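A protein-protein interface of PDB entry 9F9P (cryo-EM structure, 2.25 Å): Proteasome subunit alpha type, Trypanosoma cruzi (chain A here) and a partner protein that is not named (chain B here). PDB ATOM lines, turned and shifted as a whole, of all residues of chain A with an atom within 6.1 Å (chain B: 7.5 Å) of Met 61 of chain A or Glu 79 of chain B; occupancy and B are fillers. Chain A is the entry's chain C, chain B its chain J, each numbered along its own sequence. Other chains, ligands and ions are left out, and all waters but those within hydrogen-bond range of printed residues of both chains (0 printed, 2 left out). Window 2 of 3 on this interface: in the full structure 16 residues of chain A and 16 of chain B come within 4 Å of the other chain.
OG of Ser 67 of chain A is in hydrogen-bond range of OE1 of Glu 79 of chain B, at 2.5 Å.
O of Glu 79 of chain B sits at hydrogen-bond distance from N of Asp 63 of chain A, at 3.0 Å.
The side-chain carboxylate of Glu 62 of chain A lies within hydrogen-bond range of the backbone NH of Glu 81 of chain B (3.3 Å).
The side-chain hydroxyl (OH) of Tyr 74 of chain B is in hydrogen-bond range of the guanidinium group (NH2) of Arg 80 of chain B (3.3 Å).
The side-chain carboxylate (OE2) of Glu 78 of chain B lies within salt-bridge range of the guanidinium group (NE) of Arg 80 of chain B (3.0 Å).
The side-chain amino group (NZ) of Lys 64 of chain A is in hydrogen-bond range of the backbone carbonyl oxygen (O) of Met 61 of chain A.
Printed residues of chain A that touch a printed residue of chain B: Met 61, Glu 62, Asp 63, Ile 66, Ser 67 and Arg 97.
Of the 9 printed residues of chain B, 4 touch a printed residue of chain A.
Along chain B the printed residues that touch a printed residue of chain A span positions 76 to 81.
Among the printed residues, 9 pairs touch across the chains.
Among the printed residues, no Asp or Glu carboxylate lies within 4 Å of a Lys or Arg side-chain nitrogen of the other chain.
Met 61 of chain A touches Glu 79 of chain B.
N of Glu 62 of chain A touches O of Glu 79 of chain B, 3.6 Å away.
Arg 80 of chain B touches Glu 62 of chain A (CB to OE2, 3.5 Å).
Ile 66 of chain A touches Leu 76 of chain B.
Glu 79 of chain B touches Ile 66 of chain A.
Arg 97 of chain A touches Leu 76 of chain B (NH2 to O, 3.9 Å).
Of chain B, only Glu 79 (3.2 Å) comes within 4 Å of Met 61 of chain A.
Glu 79 of chain B touches just these residues of chain A: Met 61 (3.2 Å), Glu 62 (3.6 Å), Asp 63 (3.0 Å), Ile 66 (3.8 Å) and Ser 67 (2.5 Å).
Of the printed residues of chain A, Glu 81 of chain B touches Glu 62 (3.3 Å).
Of the printed residues of chain B, Ser 67 of chain A touches Glu 79.
Leu 73 of chain B touches none of the printed residues of chain A.
The nearest residue of chain A that does not touch Glu 79 of chain B is Arg 97 of chain A (5.5 Å).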
ATOM      1  N   SER A  58     -25.671  21.173   0.798  1.00  0.00           N
ATOM      2  CA  SER A  58     -25.718  20.592   2.126  1.00  0.00           C
ATOM      3  C   SER A  58     -27.170  20.388   2.569  1.00  0.00           C
ATOM      4  O   SER A  58     -28.042  21.190   2.243  1.00  0.00           O
ATOM      5  CB  SER A  58     -24.990  21.536   3.072  1.00  0.00           C
ATOM      6  OG  SER A  58     -25.039  21.097   4.426  1.00  0.00           O
ATOM      7  N   GLU A  59     -27.420  19.340   3.359  1.00  0.00           N
ATOM      8  CA  GLU A  59     -28.697  19.198   4.044  1.00  0.00           C
ATOM      9  C   GLU A  59     -28.815  20.233   5.185  1.00  0.00           C
ATOM     10  O   GLU A  59     -29.917  20.512   5.659  1.00  0.00           O
ATOM     11  CB  GLU A  59     -28.885  17.752   4.537  1.00  0.00           C
ATOM     12  CG  GLU A  59     -29.031  16.654   3.453  1.00  0.00           C
ATOM     13  CD  GLU A  59     -29.520  15.268   3.957  1.00  0.00           C
ATOM     14  OE1 GLU A  59     -28.679  14.325   4.096  1.00  0.00           O
ATOM     15  OE2 GLU A  59     -30.749  15.105   4.219  1.00  0.00           O
ATOM     16  N   ASN A  60     -27.693  20.799   5.635  1.00  0.00           N
ATOM     17  CA  ASN A  60     -27.627  21.740   6.756  1.00  0.00           C
ATOM     18  C   ASN A  60     -28.243  21.162   8.036  1.00  0.00           C
ATOM     19  O   ASN A  60     -29.069  21.812   8.661  1.00  0.00           O
ATOM     20  CB  ASN A  60     -28.222  23.105   6.418  1.00  0.00           C
ATOM     21  CG  ASN A  60     -27.857  24.176   7.437  1.00  0.00           C
ATOM     22  OD1 ASN A  60     -26.696  24.306   7.835  1.00  0.00           O
ATOM     23  ND2 ASN A  60     -28.840  24.943   7.891  1.00  0.00           N
ATOM     24  N   MET A  61     -27.778  19.981   8.466  1.00  0.00           N
ATOM     25  CA  MET A  61     -28.245  19.325   9.684  1.00  0.00           C
ATOM     26  C   MET A  61     -27.635  19.994  10.920  1.00  0.00           C
ATOM     27  O   MET A  61     -26.513  20.481  10.877  1.00  0.00           O
ATOM     28  CB  MET A  61     -27.836  17.842   9.684  1.00  0.00           C
ATOM     29  CG  MET A  61     -28.477  16.991   8.564  1.00  0.00           C
ATOM     30  SD  MET A  61     -30.306  16.976   8.579  1.00  0.00           S
ATOM     31  CE  MET A  61     -30.595  15.216   8.377  1.00  0.00           C
ATOM     32  N   GLU A  62     -28.367  19.973  12.044  1.00  0.00           N
ATOM     33  CA  GLU A  62     -27.995  20.715  13.242  1.00  0.00           C
ATOM     34  C   GLU A  62     -26.765  20.113  13.931  1.00  0.00           C
ATOM     35  O   GLU A  62     -25.921  20.876  14.385  1.00  0.00           O
ATOM     36  CB  GLU A  62     -29.222  20.832  14.148  1.00  0.00           C
ATOM     37  CG  GLU A  62     -28.984  21.594  15.444  1.00  0.00           C
ATOM     38  CD  GLU A  62     -30.096  21.506  16.495  1.00  0.00           C
ATOM     39  OE1 GLU A  62     -31.136  22.196  16.302  1.00  0.00           O
ATOM     40  OE2 GLU A  62     -29.927  20.730  17.516  1.00  0.00           O
ATOM     41  N   ASP A  63     -26.645  18.771  14.001  1.00  0.00           N
ATOM     42  CA  ASP A  63     -25.481  18.067  14.553  1.00  0.00           C
ATOM     43  C   ASP A  63     -24.689  17.377  13.434  1.00  0.00           C
ATOM     44  O   ASP A  63     -25.250  16.569  12.700  1.00  0.00           O
ATOM     45  CB  ASP A  63     -25.949  17.024  15.584  1.00  0.00           C
ATOM     46  CG  ASP A  63     -24.887  16.115  16.220  1.00  0.00           C
ATOM     47  OD1 ASP A  63     -23.689  16.184  15.848  1.00  0.00           O
ATOM     48  OD2 ASP A  63     -25.261  15.348  17.128  1.00  0.00           O
ATOM     49  N   LYS A  64     -23.372  17.622  13.338  1.00  0.00           N
ATOM     50  CA  LYS A  64     -22.608  17.229  12.155  1.00  0.00           C
ATOM     51  C   LYS A  64     -21.928  15.860  12.277  1.00  0.00           C
ATOM     52  O   LYS A  64     -21.491  15.314  11.266  1.00  0.00           O
ATOM     53  CB  LYS A  64     -21.550  18.282  11.828  1.00  0.00           C
ATOM     54  CG  LYS A  64     -22.060  19.714  11.725  1.00  0.00           C
ATOM     55  CD  LYS A  64     -22.825  20.043  10.446  1.00  0.00           C
ATOM     56  CE  LYS A  64     -23.346  21.469  10.462  1.00  0.00           C
ATOM     57  NZ  LYS A  64     -24.209  21.768   9.291  1.00  0.00           N
ATOM     58  N   ILE A  66     -23.228  12.775  12.932  1.00  0.00           N
ATOM     59  CA  ILE A  66     -24.114  11.620  12.952  1.00  0.00           C
ATOM     60  C   ILE A  66     -24.026  10.878  11.620  1.00  0.00           C
ATOM     61  O   ILE A  66     -24.151   9.652  11.603  1.00  0.00           O
ATOM     62  CB  ILE A  66     -25.570  12.036  13.257  1.00  0.00           C
ATOM     63  CG1 ILE A  66     -25.702  12.801  14.576  1.00  0.00           C
ATOM     64  CG2 ILE A  66     -26.542  10.856  13.180  1.00  0.00           C
ATOM     65  CD1 ILE A  66     -25.729  11.954  15.799  1.00  0.00           C
ATOM     66  N   SER A  67     -23.939  11.634  10.511  1.00  0.00           N
ATOM     67  CA  SER A  67     -23.884  11.041   9.187  1.00  0.00           C
ATOM     68  C   SER A  67     -23.214  11.979   8.195  1.00  0.00           C
ATOM     69  O   SER A  67     -23.517  13.166   8.157  1.00  0.00           O
ATOM     70  CB  SER A  67     -25.254  10.666   8.692  1.00  0.00           C
ATOM     71  OG  SER A  67     -26.014  11.817   8.364  1.00  0.00           O
ATOM     72  N   ARG A  97     -29.414   0.250  14.279  1.00  0.00           N
ATOM     73  CA  ARG A  97     -29.759   1.304  15.222  1.00  0.00           C
ATOM     74  C   ARG A  97     -30.826   0.852  16.213  1.00  0.00           C
ATOM     75  O   ARG A  97     -30.724   1.127  17.391  1.00  0.00           O
ATOM     76  CB  ARG A  97     -30.228   2.533  14.461  1.00  0.00           C
ATOM     77  CG  ARG A  97     -29.062   3.243  13.820  1.00  0.00           C
ATOM     78  CD  ARG A  97     -29.490   4.474  13.060  1.00  0.00           C
ATOM     79  NE  ARG A  97     -28.321   5.277  12.718  1.00  0.00           N
ATOM     80  CZ  ARG A  97     -28.360   6.345  11.918  1.00  0.00           C
ATOM     81  NH1 ARG A  97     -27.298   7.127  11.763  1.00  0.00           N
ATOM     82  NH2 ARG A  97     -29.485   6.650  11.317  1.00  0.00           N
ATOM     83  N   LEU B  73     -33.424   7.297  19.521  1.00  0.00           N
ATOM     84  CA  LEU B  73     -33.723   7.118  18.121  1.00  0.00           C
ATOM     85  C   LEU B  73     -34.062   8.402  17.385  1.00  0.00           C
ATOM     86  O   LEU B  73     -33.850   8.454  16.194  1.00  0.00           O
ATOM     87  CB  LEU B  73     -34.894   6.176  17.939  1.00  0.00           C
ATOM     88  CG  LEU B  73     -34.668   4.758  18.433  1.00  0.00           C
ATOM     89  CD1 LEU B  73     -35.987   4.043  18.291  1.00  0.00           C
ATOM     90  CD2 LEU B  73     -33.561   4.028  17.679  1.00  0.00           C
ATOM     91  N   TYR B  74     -34.642   9.386  18.050  1.00  0.00           N
ATOM     92  CA  TYR B  74     -34.950  10.679  17.448  1.00  0.00           C
ATOM     93  C   TYR B  74     -33.666  11.368  17.006  1.00  0.00           C
ATOM     94  O   TYR B  74     -33.573  11.785  15.887  1.00  0.00           O
ATOM     95  CB  TYR B  74     -35.757  11.536  18.423  1.00  0.00           C
ATOM     96  CG  TYR B  74     -36.176  12.908  17.969  1.00  0.00           C
ATOM     97  CD1 TYR B  74     -35.324  13.995  18.039  1.00  0.00           C
ATOM     98  CD2 TYR B  74     -37.451  13.148  17.518  1.00  0.00           C
ATOM     99  CE1 TYR B  74     -35.691  15.246  17.578  1.00  0.00           C
ATOM    100  CE2 TYR B  74     -37.874  14.409  17.149  1.00  0.00           C
ATOM    101  CZ  TYR B  74     -37.004  15.473  17.190  1.00  0.00           C
ATOM    102  OH  TYR B  74     -37.460  16.723  16.797  1.00  0.00           O
ATOM    103  N   LYS B  75     -32.725  11.510  17.894  1.00  0.00           N
ATOM    104  CA  LYS B  75     -31.447  12.104  17.582  1.00  0.00           C
ATOM    105  C   LYS B  75     -30.724  11.460  16.402  1.00  0.00           C
ATOM    106  O   LYS B  75     -30.098  12.196  15.664  1.00  0.00           O
ATOM    107  CB  LYS B  75     -30.523  12.007  18.800  1.00  0.00           C
ATOM    108  CG  LYS B  75     -30.931  12.932  19.930  1.00  0.00           C
ATOM    109  CD  LYS B  75     -29.922  12.990  21.055  1.00  0.00           C
ATOM    110  CE  LYS B  75     -30.360  12.098  22.201  1.00  0.00           C
ATOM    111  NZ  LYS B  75     -29.217  11.715  23.061  1.00  0.00           N
ATOM    112  N   LEU B  76     -30.792  10.132  16.202  1.00  0.00           N
ATOM    113  CA  LEU B  76     -30.119   9.500  15.064  1.00  0.00           C
ATOM    114  C   LEU B  76     -30.877   9.767  13.764  1.00  0.00           C
ATOM    115  O   LEU B  76     -30.300  10.168  12.782  1.00  0.00           O
ATOM    116  CB  LEU B  76     -29.973   7.997  15.303  1.00  0.00           C
ATOM    117  CG  LEU B  76     -29.118   7.570  16.484  1.00  0.00           C
ATOM    118  CD1 LEU B  76     -29.373   6.141  16.882  1.00  0.00           C
ATOM    119  CD2 LEU B  76     -27.663   7.687  16.152  1.00  0.00           C
ATOM    120  N   ARG B  77     -32.187   9.594  13.756  1.00  0.00           N
ATOM    121  CA  ARG B  77     -32.997   9.974  12.607  1.00  0.00           C
ATOM    122  C   ARG B  77     -32.860  11.460  12.285  1.00  0.00           C
ATOM    123  O   ARG B  77     -32.591  11.782  11.159  1.00  0.00           O
ATOM    124  CB  ARG B  77     -34.480   9.708  12.829  1.00  0.00           C
ATOM    125  CG  ARG B  77     -34.936   8.261  12.837  1.00  0.00           C
ATOM    126  CD  ARG B  77     -36.470   8.318  12.664  1.00  0.00           C
ATOM    127  NE  ARG B  77     -37.212   9.166  13.613  1.00  0.00           N
ATOM    128  CZ  ARG B  77     -37.602   8.783  14.846  1.00  0.00           C
ATOM    129  NH1 ARG B  77     -37.336   7.572  15.289  1.00  0.00           N
ATOM    130  NH2 ARG B  77     -38.261   9.608  15.642  1.00  0.00           N
ATOM    131  N   GLU B  78     -33.060  12.381  13.225  1.00  0.00           N
ATOM    132  CA  GLU B  78     -33.274  13.787  12.892  1.00  0.00           C
ATOM    133  C   GLU B  78     -32.000  14.623  12.955  1.00  0.00           C
ATOM    134  O   GLU B  78     -31.992  15.767  12.518  1.00  0.00           O
ATOM    135  CB  GLU B  78     -34.235  14.472  13.861  1.00  0.00           C
ATOM    136  CG  GLU B  78     -35.631  13.859  13.934  1.00  0.00           C
ATOM    137  CD  GLU B  78     -36.835  14.780  13.683  1.00  0.00           C
ATOM    138  OE1 GLU B  78     -37.996  14.271  13.777  1.00  0.00           O
ATOM    139  OE2 GLU B  78     -36.644  15.966  13.326  1.00  0.00           O
ATOM    140  N   GLU B  79     -30.960  14.078  13.581  1.00  0.00           N
ATOM    141  CA  GLU B  79     -29.705  14.782  13.760  1.00  0.00           C
ATOM    142  C   GLU B  79     -29.866  16.148  14.434  1.00  0.00           C
ATOM    143  O   GLU B  79     -29.175  17.087  14.061  1.00  0.00           O
ATOM    144  CB  GLU B  79     -28.982  14.899  12.429  1.00  0.00           C
ATOM    145  CG  GLU B  79     -28.878  13.565  11.720  1.00  0.00           C
ATOM    146  CD  GLU B  79     -27.948  13.431  10.505  1.00  0.00           C
ATOM    147  OE1 GLU B  79     -27.902  12.306   9.940  1.00  0.00           O
ATOM    148  OE2 GLU B  79     -27.294  14.418  10.097  1.00  0.00           O
ATOM    149  N   ARG B  80     -30.659  16.216  15.495  1.00  0.00           N
ATOM    150  CA  ARG B  80     -30.800  17.419  16.294  1.00  0.00           C
ATOM    151  C   ARG B  80     -31.385  17.023  17.644  1.00  0.00           C
ATOM    152  O   ARG B  80     -31.911  15.916  17.786  1.00  0.00           O
ATOM    153  CB  ARG B  80     -31.680  18.462  15.593  1.00  0.00           C
ATOM    154  CG  ARG B  80     -33.096  17.981  15.342  1.00  0.00           C
ATOM    155  CD  ARG B  80     -34.060  19.012  14.738  1.00  0.00           C
ATOM    156  NE  ARG B  80     -35.396  18.460  14.492  1.00  0.00           N
ATOM    157  CZ  ARG B  80     -36.490  19.194  14.470  1.00  0.00           C
ATOM    158  NH1 ARG B  80     -36.406  20.468  14.764  1.00  0.00           N
ATOM    159  NH2 ARG B  80     -37.679  18.691  14.167  1.00  0.00           N
ATOM    160  N   GLU B  81     -31.254  17.890  18.647  1.00  0.00           N
ATOM    161  CA  GLU B  81     -31.939  17.711  19.927  1.00  0.00           C
ATOM    162  C   GLU B  81     -33.406  18.105  19.807  1.00  0.00           C
ATOM    163  O   GLU B  81     -33.731  19.034  19.090  1.00  0.00           O
ATOM    164  CB  GLU B  81     -31.311  18.605  20.994  1.00  0.00           C
ATOM    165  CG  GLU B  81     -29.846  18.291  21.267  1.00  0.00           C
ATOM    166  CD  GLU B  81     -29.562  16.973  22.002  1.00  0.00           C
ATOM    167  OE1 GLU B  81     -28.364  16.631  22.156  1.00  0.00           O
ATOM    168  OE2 GLU B  81     -30.528  16.289  22.442  1.00  0.00           O
